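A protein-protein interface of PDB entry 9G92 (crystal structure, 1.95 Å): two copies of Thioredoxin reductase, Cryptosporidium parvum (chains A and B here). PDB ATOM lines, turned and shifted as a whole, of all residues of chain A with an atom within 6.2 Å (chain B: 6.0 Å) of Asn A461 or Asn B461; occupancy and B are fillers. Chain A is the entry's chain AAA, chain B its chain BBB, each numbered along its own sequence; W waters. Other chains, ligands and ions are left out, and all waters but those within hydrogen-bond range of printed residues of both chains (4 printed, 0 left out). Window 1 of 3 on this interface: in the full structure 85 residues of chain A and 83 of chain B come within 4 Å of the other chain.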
ATOM      1  N   THR A 376     -12.336  13.120 -12.316  1.00  0.00           N
ATOM      2  CA  THR A 376     -12.234  13.348 -13.756  1.00  0.00           C
ATOM      3  C   THR A 376     -10.820  12.985 -14.165  1.00  0.00           C
ATOM      4  O   THR A 376      -9.863  13.481 -13.540  1.00  0.00           O
ATOM      5  CB  THR A 376     -12.677  14.767 -14.130  1.00  0.00           C
ATOM      6  OG1 THR A 376     -14.068  14.850 -13.861  1.00  0.00           O
ATOM      7  CG2 THR A 376     -12.446  15.079 -15.591  1.00  0.00           C
ATOM      8  N   GLU A 382     -12.253  13.973 -21.952  1.00  0.00           N
ATOM      9  CA  GLU A 382     -12.201  13.825 -20.490  1.00  0.00           C
ATOM     10  C   GLU A 382     -13.219  12.775 -20.032  1.00  0.00           C
ATOM     11  O   GLU A 382     -14.137  12.398 -20.795  1.00  0.00           O
ATOM     12  CB  GLU A 382     -12.406  15.189 -19.852  1.00  0.00           C
ATOM     13  CG  GLU A 382     -11.458  16.267 -20.361  1.00  0.00           C
ATOM     14  CD  GLU A 382     -11.725  17.641 -19.774  1.00  0.00           C
ATOM     15  OE1 GLU A 382     -12.750  17.801 -19.046  1.00  0.00           O
ATOM     16  OE2 GLU A 382     -10.891  18.538 -20.019  1.00  0.00           O
ATOM     17  N   PHE A 457     -19.677  10.349 -17.613  1.00  0.00           N
ATOM     18  CA  PHE A 457     -19.624  11.227 -18.802  1.00  0.00           C
ATOM     19  C   PHE A 457     -18.205  11.265 -19.369  1.00  0.00           C
ATOM     20  O   PHE A 457     -17.247  11.711 -18.670  1.00  0.00           O
ATOM     21  CB  PHE A 457     -20.141  12.629 -18.465  1.00  0.00           C
ATOM     22  CG  PHE A 457     -20.126  13.492 -19.697  1.00  0.00           C
ATOM     23  CD1 PHE A 457     -21.123  13.359 -20.646  1.00  0.00           C
ATOM     24  CD2 PHE A 457     -19.076  14.350 -19.950  1.00  0.00           C
ATOM     25  CE1 PHE A 457     -21.100  14.121 -21.797  1.00  0.00           C
ATOM     26  CE2 PHE A 457     -19.038  15.096 -21.116  1.00  0.00           C
ATOM     27  CZ  PHE A 457     -20.072  15.001 -22.019  1.00  0.00           C
ATOM     28  N   GLY A 459     -16.288  13.105 -22.496  1.00  0.00           N
ATOM     29  CA  GLY A 459     -16.417  14.231 -23.439  1.00  0.00           C
ATOM     30  C   GLY A 459     -15.668  15.462 -22.939  1.00  0.00           C
ATOM     31  O   GLY A 459     -14.926  15.389 -21.958  1.00  0.00           O
ATOM     32  N   PRO A 460     -15.842  16.619 -23.620  1.00  0.00           N
ATOM     33  CA  PRO A 460     -15.242  17.875 -23.178  1.00  0.00           C
ATOM     34  C   PRO A 460     -15.859  18.335 -21.856  1.00  0.00           C
ATOM     35  O   PRO A 460     -17.012  18.002 -21.579  1.00  0.00           O
ATOM     36  CB  PRO A 460     -15.569  18.891 -24.290  1.00  0.00           C
ATOM     37  CG  PRO A 460     -16.129  18.079 -25.432  1.00  0.00           C
ATOM     38  CD  PRO A 460     -16.650  16.792 -24.837  1.00  0.00           C
ATOM     39  N   ASN A 461     -15.064  19.028 -21.038  1.00  0.00           N
ATOM     40  CA  ASN A 461     -15.560  19.681 -19.798  1.00  0.00           C
ATOM     41  C   ASN A 461     -16.193  18.659 -18.842  1.00  0.00           C
ATOM     42  O   ASN A 461     -17.147  19.031 -18.168  1.00  0.00           O
ATOM     43  CB  ASN A 461     -16.598  20.754 -20.147  1.00  0.00           C
ATOM     44  CG  ASN A 461     -16.064  21.677 -21.224  1.00  0.00           C
ATOM     45  OD1 ASN A 461     -14.984  22.237 -21.058  1.00  0.00           O
ATOM     46  ND2 ASN A 461     -16.767  21.765 -22.339  1.00  0.00           N
ATOM     47  N   ALA A 462     -15.672  17.442 -18.771  1.00  0.00           N
ATOM     48  CA  ALA A 462     -16.344  16.332 -18.058  1.00  0.00           C
ATOM     49  C   ALA A 462     -16.391  16.616 -16.561  1.00  0.00           C
ATOM     50  O   ALA A 462     -17.367  16.213 -15.939  1.00  0.00           O
ATOM     51  CB  ALA A 462     -15.691  15.005 -18.343  1.00  0.00           C
ATOM     52  N   GLY A 463     -15.368  17.267 -16.002  1.00  0.00           N
ATOM     53  CA  GLY A 463     -15.356  17.645 -14.580  1.00  0.00           C
ATOM     54  C   GLY A 463     -16.410  18.712 -14.281  1.00  0.00           C
ATOM     55  O   GLY A 463     -17.050  18.639 -13.234  1.00  0.00           O
ATOM     56  N   GLU A 464     -16.547  19.704 -15.160  1.00  0.00           N
ATOM     57  CA  GLU A 464     -17.551  20.800 -15.048  1.00  0.00           C
ATOM     58  C   GLU A 464     -18.963  20.185 -15.032  1.00  0.00           C
ATOM     59  O   GLU A 464     -19.777  20.641 -14.216  1.00  0.00           O
ATOM     60  CB  GLU A 464     -17.396  21.831 -16.172  1.00  0.00           C
ATOM     61  CG  GLU A 464     -16.000  22.419 -16.264  1.00  0.00           C
ATOM     62  CD  GLU A 464     -15.456  23.111 -15.028  1.00  0.00           C
ATOM     63  OE1 GLU A 464     -16.238  23.353 -14.067  1.00  0.00           O
ATOM     64  OE2 GLU A 464     -14.243  23.440 -15.049  1.00  0.00           O
ATOM     65  N   ILE A 465     -19.232  19.190 -15.886  1.00  0.00           N
ATOM     66  CA  ILE A 465     -20.549  18.499 -15.994  1.00  0.00           C
ATOM     67  C   ILE A 465     -20.769  17.603 -14.784  1.00  0.00           C
ATOM     68  O   ILE A 465     -21.888  17.628 -14.202  1.00  0.00           O
ATOM     69  CB  ILE A 465     -20.659  17.712 -17.317  1.00  0.00           C
ATOM     70  CG1 ILE A 465     -20.646  18.664 -18.515  1.00  0.00           C
ATOM     71  CG2 ILE A 465     -21.896  16.813 -17.309  1.00  0.00           C
ATOM     72  CD1 ILE A 465     -20.448  17.984 -19.856  1.00  0.00           C
ATOM     73  N   THR A 466     -19.757  16.842 -14.391  1.00  0.00           N
ATOM     74  CA  THR A 466     -19.916  15.783 -13.364  1.00  0.00           C
ATOM     75  C   THR A 466     -20.163  16.400 -11.984  1.00  0.00           C
ATOM     76  O   THR A 466     -20.892  15.760 -11.198  1.00  0.00           O
ATOM     77  CB  THR A 466     -18.708  14.839 -13.335  1.00  0.00           C
ATOM     78  OG1 THR A 466     -18.648  14.224 -14.614  1.00  0.00           O
ATOM     79  CG2 THR A 466     -18.813  13.767 -12.271  1.00  0.00           C
ATOM     80  N   ASP A 492     -23.626  19.757 -23.926  1.00  0.00           N
ATOM     81  CA  ASP A 492     -23.478  18.287 -23.802  1.00  0.00           C
ATOM     82  C   ASP A 492     -24.268  17.793 -22.582  1.00  0.00           C
ATOM     83  O   ASP A 492     -24.891  16.737 -22.722  1.00  0.00           O
ATOM     84  CB  ASP A 492     -22.008  17.892 -23.822  1.00  0.00           C
ATOM     85  CG  ASP A 492     -21.355  18.264 -25.143  1.00  0.00           C
ATOM     86  OD1 ASP A 492     -22.072  18.244 -26.194  1.00  0.00           O
ATOM     87  OD2 ASP A 492     -20.147  18.603 -25.116  1.00  0.00           O
ATOM     88  N   GLU B 382     -20.023  33.287 -19.925  1.00  0.00           N
ATOM     89  CA  GLU B 382     -21.398  32.750 -19.977  1.00  0.00           C
ATOM     90  C   GLU B 382     -22.061  32.906 -18.605  1.00  0.00           C
ATOM     91  O   GLU B 382     -21.362  33.158 -17.580  1.00  0.00           O
ATOM     92  CB  GLU B 382     -21.345  31.292 -20.434  1.00  0.00           C
ATOM     93  CG  GLU B 382     -20.607  31.086 -21.734  1.00  0.00           C
ATOM     94  CD  GLU B 382     -20.460  29.631 -22.152  1.00  0.00           C
ATOM     95  OE1 GLU B 382     -20.858  28.728 -21.358  1.00  0.00           O
ATOM     96  OE2 GLU B 382     -19.930  29.407 -23.258  1.00  0.00           O
ATOM     97  N   PHE B 457     -24.021  30.960 -11.853  1.00  0.00           N
ATOM     98  CA  PHE B 457     -22.604  30.820 -12.241  1.00  0.00           C
ATOM     99  C   PHE B 457     -22.340  31.646 -13.504  1.00  0.00           C
ATOM    100  O   PHE B 457     -22.968  31.409 -14.561  1.00  0.00           O
ATOM    101  CB  PHE B 457     -22.218  29.354 -12.422  1.00  0.00           C
ATOM    102  CG  PHE B 457     -20.764  29.220 -12.784  1.00  0.00           C
ATOM    103  CD1 PHE B 457     -19.796  29.342 -11.799  1.00  0.00           C
ATOM    104  CD2 PHE B 457     -20.361  29.123 -14.099  1.00  0.00           C
ATOM    105  CE1 PHE B 457     -18.448  29.286 -12.122  1.00  0.00           C
ATOM    106  CE2 PHE B 457     -19.014  29.097 -14.426  1.00  0.00           C
ATOM    107  CZ  PHE B 457     -18.064  29.162 -13.435  1.00  0.00           C
ATOM    108  N   GLY B 459     -19.176  32.452 -15.936  1.00  0.00           N
ATOM    109  CA  GLY B 459     -17.846  31.942 -16.312  1.00  0.00           C
ATOM    110  C   GLY B 459     -17.891  31.071 -17.562  1.00  0.00           C
ATOM    111  O   GLY B 459     -18.907  31.032 -18.258  1.00  0.00           O
ATOM    112  N   PRO B 460     -16.769  30.376 -17.867  1.00  0.00           N
ATOM    113  CA  PRO B 460     -16.699  29.447 -18.978  1.00  0.00           C
ATOM    114  C   PRO B 460     -17.594  28.229 -18.722  1.00  0.00           C
ATOM    115  O   PRO B 460     -17.764  27.838 -17.562  1.00  0.00           O
ATOM    116  CB  PRO B 460     -15.228  28.966 -19.019  1.00  0.00           C
ATOM    117  CG  PRO B 460     -14.476  29.983 -18.167  1.00  0.00           C
ATOM    118  CD  PRO B 460     -15.488  30.463 -17.143  1.00  0.00           C
ATOM    119  N   ASN B 461     -18.158  27.665 -19.795  1.00  0.00           N
ATOM    120  CA  ASN B 461     -18.922  26.392 -19.725  1.00  0.00           C
ATOM    121  C   ASN B 461     -20.071  26.494 -18.724  1.00  0.00           C
ATOM    122  O   ASN B 461     -20.331  25.485 -18.022  1.00  0.00           O
ATOM    123  CB  ASN B 461     -17.963  25.268 -19.348  1.00  0.00           C
ATOM    124  CG  ASN B 461     -16.740  25.281 -20.242  1.00  0.00           C
ATOM    125  OD1 ASN B 461     -16.885  25.266 -21.459  1.00  0.00           O
ATOM    126  ND2 ASN B 461     -15.560  25.348 -19.661  1.00  0.00           N
ATOM    127  N   ALA B 462     -20.737  27.653 -18.625  1.00  0.00           N
ATOM    128  CA  ALA B 462     -21.712  27.900 -17.538  1.00  0.00           C
ATOM    129  C   ALA B 462     -22.915  26.966 -17.687  1.00  0.00           C
ATOM    130  O   ALA B 462     -23.462  26.545 -16.645  1.00  0.00           O
ATOM    131  CB  ALA B 462     -22.138  29.339 -17.502  1.00  0.00           C
ATOM    132  N   GLY B 463     -23.315  26.652 -18.918  1.00  0.00           N
ATOM    133  CA  GLY B 463     -24.414  25.692 -19.159  1.00  0.00           C
ATOM    134  C   GLY B 463     -24.057  24.276 -18.736  1.00  0.00           C
ATOM    135  O   GLY B 463     -24.932  23.580 -18.151  1.00  0.00           O
ATOM    136  N   GLU B 464     -22.828  23.854 -19.041  1.00  0.00           N
ATOM    137  CA  GLU B 464     -22.291  22.525 -18.665  1.00  0.00           C
ATOM    138  C   GLU B 464     -22.309  22.391 -17.132  1.00  0.00           C
ATOM    139  O   GLU B 464     -22.688  21.323 -16.674  1.00  0.00           O
ATOM    140  CB  GLU B 464     -20.897  22.289 -19.248  1.00  0.00           C
ATOM    141  CG  GLU B 464     -20.801  22.441 -20.758  1.00  0.00           C
ATOM    142  CD  GLU B 464     -21.728  21.558 -21.604  1.00  0.00           C
ATOM    143  OE1 GLU B 464     -22.342  20.593 -21.032  1.00  0.00           O
ATOM    144  OE2 GLU B 464     -21.864  21.855 -22.843  1.00  0.00           O
ATOM    145  N   ILE B 465     -21.920  23.431 -16.386  1.00  0.00           N
ATOM    146  CA  ILE B 465     -21.858  23.414 -14.894  1.00  0.00           C
ATOM    147  C   ILE B 465     -23.282  23.464 -14.337  1.00  0.00           C
ATOM    148  O   ILE B 465     -23.588  22.746 -13.366  1.00  0.00           O
ATOM    149  CB  ILE B 465     -21.000  24.584 -14.361  1.00  0.00           C
ATOM    150  CG1 ILE B 465     -19.533  24.428 -14.760  1.00  0.00           C
ATOM    151  CG2 ILE B 465     -21.147  24.741 -12.861  1.00  0.00           C
ATOM    152  CD1 ILE B 465     -18.689  25.668 -14.539  1.00  0.00           C
ATOM    153  N   THR B 466     -24.135  24.309 -14.901  1.00  0.00           N
ATOM    154  CA  THR B 466     -25.450  24.575 -14.271  1.00  0.00           C
ATOM    155  C   THR B 466     -26.362  23.344 -14.395  1.00  0.00           C
ATOM    156  O   THR B 466     -27.200  23.155 -13.486  1.00  0.00           O
ATOM    157  CB  THR B 466     -26.098  25.835 -14.857  1.00  0.00           C
ATOM    158  OG1 THR B 466     -25.237  26.944 -14.633  1.00  0.00           O
ATOM    159  CG2 THR B 466     -27.455  26.146 -14.262  1.00  0.00           C
ATOM    160  N   ASP B 492     -13.722  24.774 -12.362  1.00  0.00           N
ATOM    161  CA  ASP B 492     -14.457  25.947 -11.827  1.00  0.00           C
ATOM    162  C   ASP B 492     -15.620  25.454 -10.969  1.00  0.00           C
ATOM    163  O   ASP B 492     -15.836  26.062  -9.927  1.00  0.00           O
ATOM    164  CB  ASP B 492     -14.872  26.869 -12.963  1.00  0.00           C
ATOM    165  CG  ASP B 492     -13.678  27.469 -13.665  1.00  0.00           C
ATOM    166  OD1 ASP B 492     -12.645  27.640 -13.027  1.00  0.00           O
ATOM    167  OD2 ASP B 492     -13.796  27.733 -14.870  1.00  0.00           O
HETATM  168  O   HOH W   1     -20.488  21.376 -24.952  1.00  0.00           O
HETATM  169  O   HOH W   2     -12.794  25.395 -15.840  1.00  0.00           O
HETATM  170  O   HOH W   3     -23.729  19.501 -15.088  1.00  0.00           O
HETATM  171  O   HOH W   4     -21.706  20.810 -12.561  1.00  0.00           O
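The side-chain amide oxygen of Asn A461 is in hydrogen-bond range of the side-chain amide nitrogen of Asn B461, 3.5 Å away. OE2 of Glu A464 lies within hydrogen-bond range of N of Asp B492, 3.0 Å away. The backbone NH (N) of Asp A492 sits at hydrogen-bond distance from the side-chain carboxylate (OE2) of Glu B464 (2.9 Å).
OE1 of Glu A382 sits at hydrogen-bond distance from N of Asn A461. OE1 of Glu B382 lies within hydrogen-bond range of N of Asn B461, at 3.3 Å.
Glu B464 touches Glu A464. CD1 of Ile B465 touches OE1 of Glu A464, 3.4 Å away. OE1 of Glu B464 touches CD1 of Ile A465, at 3.4 Å.
Asn A461 touches just one residue of chain B: Asn B461 (3.5 Å). Of the printed residues of chain B, Glu A464 touches Glu B464 (3.9 Å), Ile B465 (3.4 Å) and Asp B492 (3.0 Å). Printed residues of chain B within 4 Å of Asp A492: Glu B464. Asn B461 touches just one residue of chain A: Asn A461. Of the printed residues of chain A, Glu B464 touches Glu A464, Ile A465 and Asp A492. Of the printed residues of chain A, Asp B492 touches Glu A464 (3.0 Å). The nearest residue of chain A that does not touch Asn B461 is Glu A464 (4.5 Å).
Of the 11 printed residues of chain B, 4 touch a printed residue of chain A. Of the 12 printed residues of chain A, 4 touch a printed residue of chain B. Hydrophobic or aromatic side chains of chain A within 4 Å of the printed part of chain B: Ile A465. Among the printed residues, 6 pairs touch across the chains.
Asn B461 touches its own counterpart, Asn A461. Glu B464 touches its own counterpart, Glu A464. Glu A464 touches Ile B465, and with the chains exchanged Ile A465 touches Glu B464. Glu A464 touches Asp B492, and with the chains exchanged Asp A492 touches Glu B464. 11 positions are printed for both chains.
Water W4 bridges the backbone carbonyl oxygen (O) of Glu A464 (2.5 Å) and the backbone carbonyl oxygen (O) of Ile B465 (2.8 Å). Water W2 bridges the side-chain carboxylate (OE2) of Glu A464 (2.6 Å) and the side-chain carboxylate (OD2) of Asp B492 (2.7 Å). Water W1 bridges OE2 of Glu B464 and OD2 of Asp A492. Water W3 lies within hydrogen-bond range of the backbone carbonyl oxygen (O) of Glu B464 (2.6 Å) and the backbone carbonyl oxygen (O) of Ile A465 (2.8 Å).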
